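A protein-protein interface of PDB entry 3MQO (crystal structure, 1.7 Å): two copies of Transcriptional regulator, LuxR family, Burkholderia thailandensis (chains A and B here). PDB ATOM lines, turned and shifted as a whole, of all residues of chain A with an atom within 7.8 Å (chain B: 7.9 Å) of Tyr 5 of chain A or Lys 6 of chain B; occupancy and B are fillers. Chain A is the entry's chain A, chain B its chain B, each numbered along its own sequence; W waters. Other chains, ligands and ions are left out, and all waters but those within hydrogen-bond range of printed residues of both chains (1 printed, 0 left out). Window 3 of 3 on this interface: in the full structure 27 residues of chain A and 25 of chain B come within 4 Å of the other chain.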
ATOM      1  N   ILE A   3     -13.794  -4.269  22.066  1.00  0.00           N
ATOM      2  CA  ILE A   3     -13.813  -2.820  21.692  1.00  0.00           C
ATOM      3  C   ILE A   3     -15.067  -2.472  20.883  1.00  0.00           C
ATOM      4  O   ILE A   3     -15.250  -2.975  19.766  1.00  0.00           O
ATOM      5  CB  ILE A   3     -12.552  -2.406  20.875  1.00  0.00           C
ATOM      6  CG1 ILE A   3     -11.267  -2.715  21.646  1.00  0.00           C
ATOM      7  CG2 ILE A   3     -12.610  -0.922  20.507  1.00  0.00           C
ATOM      8  CD1 ILE A   3      -9.986  -2.400  20.866  1.00  0.00           C
ATOM      9  N   ASP A   4     -15.931  -1.627  21.442  1.00  0.00           N
ATOM     10  CA  ASP A   4     -17.124  -1.186  20.716  1.00  0.00           C
ATOM     11  C   ASP A   4     -16.784  -0.006  19.809  1.00  0.00           C
ATOM     12  O   ASP A   4     -15.646   0.466  19.815  1.00  0.00           O
ATOM     13  CB  ASP A   4     -18.312  -0.890  21.647  1.00  0.00           C
ATOM     14  CG  ASP A   4     -18.044   0.230  22.646  1.00  0.00           C
ATOM     15  OD1 ASP A   4     -18.754   0.250  23.676  1.00  0.00           O
ATOM     16  OD2 ASP A   4     -17.165   1.092  22.428  1.00  0.00           O
ATOM     17  N   TYR A   5     -17.758   0.454  19.027  1.00  0.00           N
ATOM     18  CA  TYR A   5     -17.475   1.471  18.000  1.00  0.00           C
ATOM     19  C   TYR A   5     -17.099   2.819  18.590  1.00  0.00           C
ATOM     20  O   TYR A   5     -16.261   3.541  18.004  1.00  0.00           O
ATOM     21  CB  TYR A   5     -18.617   1.607  16.989  1.00  0.00           C
ATOM     22  CG  TYR A   5     -18.859   0.345  16.192  1.00  0.00           C
ATOM     23  CD1 TYR A   5     -17.944  -0.072  15.226  1.00  0.00           C
ATOM     24  CD2 TYR A   5     -19.996  -0.427  16.398  1.00  0.00           C
ATOM     25  CE1 TYR A   5     -18.149  -1.222  14.499  1.00  0.00           C
ATOM     26  CE2 TYR A   5     -20.217  -1.588  15.666  1.00  0.00           C
ATOM     27  CZ  TYR A   5     -19.286  -1.975  14.715  1.00  0.00           C
ATOM     28  OH  TYR A   5     -19.481  -3.118  13.973  1.00  0.00           O
ATOM     29  N   LYS A   6     -17.694   3.133  19.740  1.00  0.00           N
ATOM     30  CA  LYS A   6     -17.397   4.356  20.482  1.00  0.00           C
ATOM     31  C   LYS A   6     -15.962   4.357  20.991  1.00  0.00           C
ATOM     32  O   LYS A   6     -15.250   5.329  20.806  1.00  0.00           O
ATOM     33  CB  LYS A   6     -18.376   4.542  21.649  1.00  0.00           C
ATOM     34  CG  LYS A   6     -18.090   5.784  22.476  1.00  0.00           C
ATOM     35  CD  LYS A   6     -19.299   6.211  23.277  1.00  0.00           C
ATOM     36  CE  LYS A   6     -19.043   7.552  23.958  1.00  0.00           C
ATOM     37  NZ  LYS A   6     -20.195   7.996  24.792  1.00  0.00           N
ATOM     38  N   THR A   7     -15.555   3.264  21.635  1.00  0.00           N
ATOM     39  CA  THR A   7     -14.182   3.107  22.108  1.00  0.00           C
ATOM     40  C   THR A   7     -13.180   3.156  20.942  1.00  0.00           C
ATOM     41  O   THR A   7     -12.153   3.823  21.042  1.00  0.00           O
ATOM     42  CB  THR A   7     -14.002   1.816  22.922  1.00  0.00           C
ATOM     43  OG1 THR A   7     -14.913   1.829  24.024  1.00  0.00           O
ATOM     44  CG2 THR A   7     -12.593   1.723  23.461  1.00  0.00           C
ATOM     45  N   ALA A   8     -13.495   2.468  19.843  1.00  0.00           N
ATOM     46  CA  ALA A   8     -12.672   2.544  18.634  1.00  0.00           C
ATOM     47  C   ALA A   8     -12.450   3.989  18.183  1.00  0.00           C
ATOM     48  O   ALA A   8     -11.309   4.400  17.957  1.00  0.00           O
ATOM     49  CB  ALA A   8     -13.292   1.739  17.507  1.00  0.00           C
ATOM     50  N   PHE A   9     -13.541   4.739  18.052  1.00  0.00           N
ATOM     51  CA  PHE A   9     -13.477   6.135  17.619  1.00  0.00           C
ATOM     52  C   PHE A   9     -12.519   6.903  18.520  1.00  0.00           C
ATOM     53  O   PHE A   9     -11.648   7.611  18.039  1.00  0.00           O
ATOM     54  CB  PHE A   9     -14.870   6.766  17.628  1.00  0.00           C
ATOM     55  CG  PHE A   9     -14.903   8.216  17.194  1.00  0.00           C
ATOM     56  CD1 PHE A   9     -14.962   8.547  15.846  1.00  0.00           C
ATOM     57  CD2 PHE A   9     -14.917   9.237  18.139  1.00  0.00           C
ATOM     58  CE1 PHE A   9     -15.003   9.890  15.434  1.00  0.00           C
ATOM     59  CE2 PHE A   9     -14.980  10.580  17.745  1.00  0.00           C
ATOM     60  CZ  PHE A   9     -15.022  10.910  16.393  1.00  0.00           C
ATOM     61  N   HIS A  10     -12.674   6.730  19.828  1.00  0.00           N
ATOM     62  CA  HIS A  10     -11.898   7.518  20.772  1.00  0.00           C
ATOM     63  C   HIS A  10     -10.448   7.057  20.960  1.00  0.00           C
ATOM     64  O   HIS A  10      -9.591   7.883  21.266  1.00  0.00           O
ATOM     65  CB  HIS A  10     -12.637   7.657  22.108  1.00  0.00           C
ATOM     66  CG  HIS A  10     -13.784   8.621  22.058  1.00  0.00           C
ATOM     67  ND1 HIS A  10     -13.619   9.959  21.762  1.00  0.00           N
ATOM     68  CD2 HIS A  10     -15.110   8.443  22.259  1.00  0.00           C
ATOM     69  CE1 HIS A  10     -14.794  10.563  21.790  1.00  0.00           C
ATOM     70  NE2 HIS A  10     -15.715   9.667  22.092  1.00  0.00           N
ATOM     71  N   LEU A  11     -10.182   5.763  20.783  1.00  0.00           N
ATOM     72  CA  LEU A  11      -8.833   5.203  20.931  1.00  0.00           C
ATOM     73  C   LEU A  11      -8.004   5.320  19.643  1.00  0.00           C
ATOM     74  O   LEU A  11      -6.794   5.119  19.674  1.00  0.00           O
ATOM     75  CB  LEU A  11      -8.899   3.717  21.363  1.00  0.00           C
ATOM     76  CG  LEU A  11      -7.624   2.875  21.600  1.00  0.00           C
ATOM     77  CD1 LEU A  11      -6.991   3.169  22.970  1.00  0.00           C
ATOM     78  CD2 LEU A  11      -7.907   1.368  21.505  1.00  0.00           C
ATOM     79  N   LEU A  16      -9.893  11.745  14.237  1.00  0.00           N
ATOM     80  CA  LEU A  16     -11.145  11.431  13.559  1.00  0.00           C
ATOM     81  C   LEU A  16     -12.149  12.501  13.849  1.00  0.00           C
ATOM     82  O   LEU A  16     -12.159  13.060  14.960  1.00  0.00           O
ATOM     83  CB  LEU A  16     -11.740  10.109  14.038  1.00  0.00           C
ATOM     84  CG  LEU A  16     -10.981   8.854  13.650  1.00  0.00           C
ATOM     85  CD1 LEU A  16     -11.677   7.646  14.288  1.00  0.00           C
ATOM     86  CD2 LEU A  16     -10.837   8.765  12.106  1.00  0.00           C
ATOM     87  N   LEU A  18     -16.442  13.555  13.137  1.00  0.00           N
ATOM     88  CA  LEU A  18     -17.796  13.502  12.572  1.00  0.00           C
ATOM     89  C   LEU A  18     -18.197  14.938  12.325  1.00  0.00           C
ATOM     90  O   LEU A  18     -18.262  15.721  13.262  1.00  0.00           O
ATOM     91  CB  LEU A  18     -18.780  12.832  13.527  1.00  0.00           C
ATOM     92  CG  LEU A  18     -18.291  11.504  14.075  1.00  0.00           C
ATOM     93  CD1 LEU A  18     -19.388  10.822  14.882  1.00  0.00           C
ATOM     94  CD2 LEU A  18     -17.817  10.567  12.953  1.00  0.00           C
ATOM     95  N   ILE B   3     -24.391  11.226  12.417  1.00  0.00           N
ATOM     96  CA  ILE B   3     -23.578   9.993  12.193  1.00  0.00           C
ATOM     97  C   ILE B   3     -23.239   9.356  13.542  1.00  0.00           C
ATOM     98  O   ILE B   3     -22.533   9.963  14.352  1.00  0.00           O
ATOM     99  CB  ILE B   3     -22.255  10.295  11.417  1.00  0.00           C
ATOM    100  CG1 ILE B   3     -22.538  11.034  10.110  1.00  0.00           C
ATOM    101  CG2 ILE B   3     -21.454   9.001  11.150  1.00  0.00           C
ATOM    102  CD1 ILE B   3     -21.279  11.480   9.372  1.00  0.00           C
ATOM    103  N   ASP B   4     -23.736   8.146  13.799  1.00  0.00           N
ATOM    104  CA  ASP B   4     -23.357   7.463  15.038  1.00  0.00           C
ATOM    105  C   ASP B   4     -21.999   6.770  14.892  1.00  0.00           C
ATOM    106  O   ASP B   4     -21.383   6.817  13.814  1.00  0.00           O
ATOM    107  CB  ASP B   4     -24.473   6.549  15.593  1.00  0.00           C
ATOM    108  CG  ASP B   4     -24.739   5.314  14.746  1.00  0.00           C
ATOM    109  OD1 ASP B   4     -23.997   5.018  13.794  1.00  0.00           O
ATOM    110  OD2 ASP B   4     -25.720   4.607  15.058  1.00  0.00           O
ATOM    111  N   TYR B   5     -21.504   6.167  15.969  1.00  0.00           N
ATOM    112  CA  TYR B   5     -20.134   5.640  15.924  1.00  0.00           C
ATOM    113  C   TYR B   5     -20.003   4.432  15.017  1.00  0.00           C
ATOM    114  O   TYR B   5     -18.939   4.235  14.407  1.00  0.00           O
ATOM    115  CB  TYR B   5     -19.557   5.356  17.314  1.00  0.00           C
ATOM    116  CG  TYR B   5     -19.383   6.595  18.159  1.00  0.00           C
ATOM    117  CD1 TYR B   5     -18.412   7.546  17.851  1.00  0.00           C
ATOM    118  CD2 TYR B   5     -20.180   6.809  19.273  1.00  0.00           C
ATOM    119  CE1 TYR B   5     -18.261   8.690  18.623  1.00  0.00           C
ATOM    120  CE2 TYR B   5     -20.030   7.947  20.058  1.00  0.00           C
ATOM    121  CZ  TYR B   5     -19.059   8.874  19.728  1.00  0.00           C
ATOM    122  OH  TYR B   5     -18.903  10.003  20.502  1.00  0.00           O
ATOM    123  N   LYS B   6     -21.068   3.634  14.951  1.00  0.00           N
ATOM    124  CA  LYS B   6     -21.130   2.475  14.067  1.00  0.00           C
ATOM    125  C   LYS B   6     -21.030   2.872  12.595  1.00  0.00           C
ATOM    126  O   LYS B   6     -20.217   2.311  11.874  1.00  0.00           O
ATOM    127  CB  LYS B   6     -22.377   1.618  14.330  1.00  0.00           C
ATOM    128  CG  LYS B   6     -22.472   0.410  13.405  1.00  0.00           C
ATOM    129  CD  LYS B   6     -23.410  -0.644  13.950  1.00  0.00           C
ATOM    130  CE  LYS B   6     -23.406  -1.871  13.041  1.00  0.00           C
ATOM    131  NZ  LYS B   6     -24.651  -2.693  13.152  1.00  0.00           N
ATOM    132  N   THR B   7     -21.843   3.835  12.155  1.00  0.00           N
ATOM    133  CA  THR B   7     -21.833   4.341  10.783  1.00  0.00           C
ATOM    134  C   THR B   7     -20.490   5.002  10.450  1.00  0.00           C
ATOM    135  O   THR B   7     -19.988   4.902   9.337  1.00  0.00           O
ATOM    136  CB  THR B   7     -22.988   5.363  10.568  1.00  0.00           C
ATOM    137  OG1 THR B   7     -24.229   4.789  10.998  1.00  0.00           O
ATOM    138  CG2 THR B   7     -23.109   5.762   9.104  1.00  0.00           C
ATOM    139  N   ALA B   8     -19.933   5.722  11.430  1.00  0.00           N
ATOM    140  CA  ALA B   8     -18.627   6.383  11.223  1.00  0.00           C
ATOM    141  C   ALA B   8     -17.571   5.328  10.874  1.00  0.00           C
ATOM    142  O   ALA B   8     -16.807   5.480   9.902  1.00  0.00           O
ATOM    143  CB  ALA B   8     -18.205   7.193  12.449  1.00  0.00           C
ATOM    144  N   PHE B   9     -17.563   4.258  11.665  1.00  0.00           N
ATOM    145  CA  PHE B   9     -16.667   3.122  11.460  1.00  0.00           C
ATOM    146  C   PHE B   9     -16.836   2.556  10.053  1.00  0.00           C
ATOM    147  O   PHE B   9     -15.863   2.428   9.301  1.00  0.00           O
ATOM    148  CB  PHE B   9     -16.914   2.039  12.509  1.00  0.00           C
ATOM    149  CG  PHE B   9     -16.046   0.809  12.336  1.00  0.00           C
ATOM    150  CD1 PHE B   9     -14.768   0.766  12.883  1.00  0.00           C
ATOM    151  CD2 PHE B   9     -16.523  -0.304  11.646  1.00  0.00           C
ATOM    152  CE1 PHE B   9     -13.958  -0.373  12.729  1.00  0.00           C
ATOM    153  CE2 PHE B   9     -15.730  -1.456  11.505  1.00  0.00           C
ATOM    154  CZ  PHE B   9     -14.448  -1.491  12.055  1.00  0.00           C
ATOM    155  N   HIS B  10     -18.075   2.251   9.692  1.00  0.00           N
ATOM    156  CA  HIS B  10     -18.336   1.628   8.403  1.00  0.00           C
ATOM    157  C   HIS B  10     -18.210   2.523   7.170  1.00  0.00           C
ATOM    158  O   HIS B  10     -17.972   2.011   6.073  1.00  0.00           O
ATOM    159  CB  HIS B  10     -19.658   0.876   8.424  1.00  0.00           C
ATOM    160  CG  HIS B  10     -19.592  -0.394   9.211  1.00  0.00           C
ATOM    161  ND1 HIS B  10     -18.830  -1.473   8.815  1.00  0.00           N
ATOM    162  CD2 HIS B  10     -20.169  -0.750  10.382  1.00  0.00           C
ATOM    163  CE1 HIS B  10     -18.959  -2.446   9.699  1.00  0.00           C
ATOM    164  NE2 HIS B  10     -19.762  -2.032  10.661  1.00  0.00           N
ATOM    165  N   LEU B  11     -18.390   3.827   7.326  1.00  0.00           N
ATOM    166  CA  LEU B  11     -18.294   4.712   6.168  1.00  0.00           C
ATOM    167  C   LEU B  11     -16.932   5.411   6.057  1.00  0.00           C
ATOM    168  O   LEU B  11     -16.690   6.130   5.110  1.00  0.00           O
ATOM    169  CB  LEU B  11     -19.470   5.705   6.118  1.00  0.00           C
ATOM    170  CG  LEU B  11     -19.414   7.120   6.678  1.00  0.00           C
ATOM    171  CD1 LEU B  11     -18.456   7.204   7.831  1.00  0.00           C
ATOM    172  CD2 LEU B  11     -19.048   8.156   5.624  1.00  0.00           C
ATOM    173  N   ALA B  12     -16.055   5.169   7.029  1.00  0.00           N
ATOM    174  CA  ALA B  12     -14.747   5.824   7.083  1.00  0.00           C
ATOM    175  C   ALA B  12     -13.990   5.699   5.777  1.00  0.00           C
ATOM    176  O   ALA B  12     -14.000   4.641   5.163  1.00  0.00           O
ATOM    177  CB  ALA B  12     -13.908   5.242   8.237  1.00  0.00           C
ATOM    178  N   LEU B  16     -10.436   0.407   8.491  1.00  0.00           N
ATOM    179  CA  LEU B  16     -10.409   0.326   9.946  1.00  0.00           C
ATOM    180  C   LEU B  16     -10.550  -1.107  10.376  1.00  0.00           C
ATOM    181  O   LEU B  16     -11.277  -1.882   9.740  1.00  0.00           O
ATOM    182  CB  LEU B  16     -11.559   1.116  10.561  1.00  0.00           C
ATOM    183  CG  LEU B  16     -11.433   2.623  10.384  1.00  0.00           C
ATOM    184  CD1 LEU B  16     -12.642   3.301  10.959  1.00  0.00           C
ATOM    185  CD2 LEU B  16     -10.126   3.138  11.025  1.00  0.00           C
ATOM    186  N   LEU B  18     -10.941  -3.484  14.130  1.00  0.00           N
ATOM    187  CA  LEU B  18     -10.920  -3.800  15.557  1.00  0.00           C
ATOM    188  C   LEU B  18     -10.270  -5.169  15.644  1.00  0.00           C
ATOM    189  O   LEU B  18     -10.804  -6.140  15.095  1.00  0.00           O
ATOM    190  CB  LEU B  18     -12.343  -3.843  16.146  1.00  0.00           C
ATOM    191  CG  LEU B  18     -13.213  -2.639  15.796  1.00  0.00           C
ATOM    192  CD1 LEU B  18     -14.547  -2.669  16.543  1.00  0.00           C
ATOM    193  CD2 LEU B  18     -12.454  -1.345  16.115  1.00  0.00           C
ATOM    194  N   GLU B  25     -11.342  -8.748  14.143  1.00  0.00           N
ATOM    195  CA  GLU B  25     -12.643  -9.063  14.753  1.00  0.00           C
ATOM    196  C   GLU B  25     -13.761  -8.301  14.048  1.00  0.00           C
ATOM    197  O   GLU B  25     -14.919  -8.760  13.989  1.00  0.00           O
ATOM    198  CB  GLU B  25     -12.649  -8.732  16.252  1.00  0.00           C
ATOM    199  CG  GLU B  25     -11.541  -9.392  17.068  1.00  0.00           C
ATOM    200  CD  GLU B  25     -11.843 -10.827  17.438  1.00  0.00           C
ATOM    201  OE1 GLU B  25     -12.354 -11.057  18.560  1.00  0.00           O
ATOM    202  OE2 GLU B  25     -11.569 -11.732  16.613  1.00  0.00           O
ATOM    203  N   ASP B  26     -13.438  -7.095  13.586  1.00  0.00           N
ATOM    204  CA  ASP B  26     -14.385  -6.309  12.800  1.00  0.00           C
ATOM    205  C   ASP B  26     -13.590  -5.412  11.880  1.00  0.00           C
ATOM    206  O   ASP B  26     -12.451  -5.047  12.188  1.00  0.00           O
ATOM    207  CB  ASP B  26     -15.310  -5.490  13.714  1.00  0.00           C
ATOM    208  CG  ASP B  26     -16.602  -5.021  13.020  1.00  0.00           C
ATOM    209  OD1 ASP B  26     -16.813  -5.273  11.813  1.00  0.00           O
ATOM    210  OD2 ASP B  26     -17.442  -4.418  13.714  1.00  0.00           O
ATOM    211  N   CYS B  27     -14.171  -5.101  10.729  1.00  0.00           N
ATOM    212  CA  CYS B  27     -13.527  -4.185   9.788  1.00  0.00           C
ATOM    213  C   CYS B  27     -14.556  -3.503   8.928  1.00  0.00           C
ATOM    214  O   CYS B  27     -15.700  -3.891   8.926  1.00  0.00           O
ATOM    215  CB  CYS B  27     -12.493  -4.908   8.906  1.00  0.00           C
ATOM    216  SG  CYS B  27     -13.186  -6.000   7.596  1.00  0.00           S
ATOM    217  N   ASN B  28     -14.162  -2.435   8.243  1.00  0.00           N
ATOM    218  CA  ASN B  28     -15.112  -1.738   7.371  1.00  0.00           C
ATOM    219  C   ASN B  28     -14.931  -2.130   5.890  1.00  0.00           C
ATOM    220  O   ASN B  28     -14.007  -2.912   5.543  1.00  0.00           O
ATOM    221  CB  ASN B  28     -15.041  -0.209   7.596  1.00  0.00           C
ATOM    222  CG  ASN B  28     -13.680   0.382   7.264  1.00  0.00           C
ATOM    223  OD1 ASN B  28     -12.791  -0.280   6.737  1.00  0.00           O
ATOM    224  ND2 ASN B  28     -13.529   1.672   7.556  1.00  0.00           N
ATOM    225  N   ARG B  39     -16.010  -8.124   3.252  1.00  0.00           N
ATOM    226  CA  ARG B  39     -15.842  -8.004   4.700  1.00  0.00           C
ATOM    227  C   ARG B  39     -15.875  -9.387   5.326  1.00  0.00           C
ATOM    228  O   ARG B  39     -15.066  -9.691   6.194  1.00  0.00           O
ATOM    229  CB  ARG B  39     -16.958  -7.158   5.302  1.00  0.00           C
ATOM    230  CG  ARG B  39     -16.582  -5.745   5.597  1.00  0.00           C
ATOM    231  CD  ARG B  39     -17.685  -5.053   6.419  1.00  0.00           C
ATOM    232  NE  ARG B  39     -17.907  -5.701   7.718  1.00  0.00           N
ATOM    233  CZ  ARG B  39     -19.069  -6.206   8.126  1.00  0.00           C
ATOM    234  NH1 ARG B  39     -19.162  -6.774   9.322  1.00  0.00           N
ATOM    235  NH2 ARG B  39     -20.147  -6.133   7.354  1.00  0.00           N
ATOM    236  N   ILE B  43     -13.508 -11.127   8.510  1.00  0.00           N
ATOM    237  CA  ILE B  43     -13.961 -11.320   9.888  1.00  0.00           C
ATOM    238  C   ILE B  43     -13.432 -12.643  10.452  1.00  0.00           C
ATOM    239  O   ILE B  43     -13.752 -13.727   9.952  1.00  0.00           O
ATOM    240  CB  ILE B  43     -15.511 -11.248  10.018  1.00  0.00           C
ATOM    241  CG1 ILE B  43     -16.038  -9.935   9.406  1.00  0.00           C
ATOM    242  CG2 ILE B  43     -15.964 -11.455  11.480  1.00  0.00           C
ATOM    243  CD1 ILE B  43     -15.664  -8.688  10.165  1.00  0.00           C
ATOM    244  N   VAL B 107      -6.990  -0.907  17.870  1.00  0.00           N
ATOM    245  CA  VAL B 107      -7.607  -0.271  16.709  1.00  0.00           C
ATOM    246  C   VAL B 107      -6.506  -0.025  15.681  1.00  0.00           C
ATOM    247  O   VAL B 107      -5.471   0.593  16.006  1.00  0.00           O
ATOM    248  CB  VAL B 107      -8.334   1.047  17.109  1.00  0.00           C
ATOM    249  CG1 VAL B 107      -8.843   1.805  15.888  1.00  0.00           C
ATOM    250  CG2 VAL B 107      -9.495   0.747  18.067  1.00  0.00           C
HETATM  251  O   HOH W   1     -16.215   4.131  15.375  1.00  0.00           O
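Water W1 bridges O of Tyr 5 of chain A (2.7 Å) and O of Tyr 5 of chain B (2.9 Å).
Of the 19 printed residues of chain B, 9 touch a printed residue of chain A.
Hydrophobic or aromatic side chains of chain B within 4 Å of the printed part of chain A: Tyr 5, Ala 8, Phe 9, His 10, Leu 18 and Val 107.
Among the printed residues, 14 pairs touch across the chains.
Among the printed residues, no Asp or Glu carboxylate lies within 4 Å of a Lys or Arg side-chain nitrogen of the other chain.
Ile 3 of chain A touches Leu 18 of chain B, and with the chains exchanged Leu 18 of chain A touches Ile 3 of chain B.
Tyr 5 of chain B touches its own counterpart, Tyr 5 of chain A.
Tyr 5 of chain A touches Phe 9 of chain B, and with the chains exchanged Phe 9 of chain A touches Tyr 5 of chain B.
Tyr 5 of chain A touches His 10 of chain B, and with the chains exchanged His 10 of chain A touches Tyr 5 of chain B.
The side-chain hydroxyl (OH) of Tyr 5 of chain A is in hydrogen-bond range of a ring nitrogen (NE2) of His 10 of chain B, 3.5 Å away.
OH of Tyr 5 of chain A lies within hydrogen-bond range of OD2 of Asp 26 of chain B, at 2.4 Å.
N of Lys 6 of chain A sits close to OD2 of Asp 4 of chain A, at 3.4 Å.
The side-chain carboxylate (OD1) of Asp 4 of chain B lies close to the backbone NH (N) of Lys 6 of chain B, at 3.4 Å.
The side-chain amide nitrogen of Asn 28 of chain B lies within hydrogen-bond range of the backbone carbonyl oxygen of Phe 9 of chain B (3.0 Å).
The backbone carbonyl oxygen of Leu 18 of chain B is in hydrogen-bond range of the backbone NH of Glu 25 of chain B (2.8 Å).
N of Leu 18 of chain B is in hydrogen-bond range of O of Asp 26 of chain B (2.9 Å).
The side-chain carboxylate (OD1) of Asp 26 of chain B lies within salt-bridge range of the guanidinium group (NH1) of Arg 39 of chain B, at 3.7 Å.
Tyr 5 of chain A touches five residues of chain B.
Of chain A, only Tyr 5 comes within 4 Å of Lys 6 of chain B.
Of the printed residues of chain A, Ala 8 of chain B touches Leu 18 (3.4 Å).
Of the printed residues of chain A, Asp 26 of chain B touches Tyr 5 (2.4 Å).
Leu 16 of chain A touches none of the printed residues of chain B.
The nearest residue of chain A that does not touch Lys 6 of chain B is Lys 6 of chain A (5.9 Å).
The nearest printed residue of chain A that does not touch Ala 8 of chain B is Phe 9 of chain A (4.9 Å).
Among the printed residues, merely in contact across the chains: Leu 18 of chain A with Ile 3 of chain B (3.3 Å), Ile 3 of chain A with Leu 18 of chain B (3.3 Å), Tyr 5 of chain A with Phe 9 of chain B (3.4 Å), Phe 9 of chain A with Tyr 5 of chain B (3.4 Å), Leu 18 of chain A with Ala 8 of chain B (3.4 Å), Ala 8 of chain A with Leu 18 of chain B (3.5 Å), His 10 of chain A with Tyr 5 of chain B (3.6 Å), Ala 8 of chain A with Val 107 of chain B (3.7 Å), Tyr 5 of chain A with Tyr 5 of chain B (3.7 Å), Lys 6 of chain A with Tyr 5 of chain B (3.7 Å), Tyr 5 of chain A with Lys 6 of chain B (3.7 Å) and Leu 11 of chain A with Val 107 of chain B (3.8 Å).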
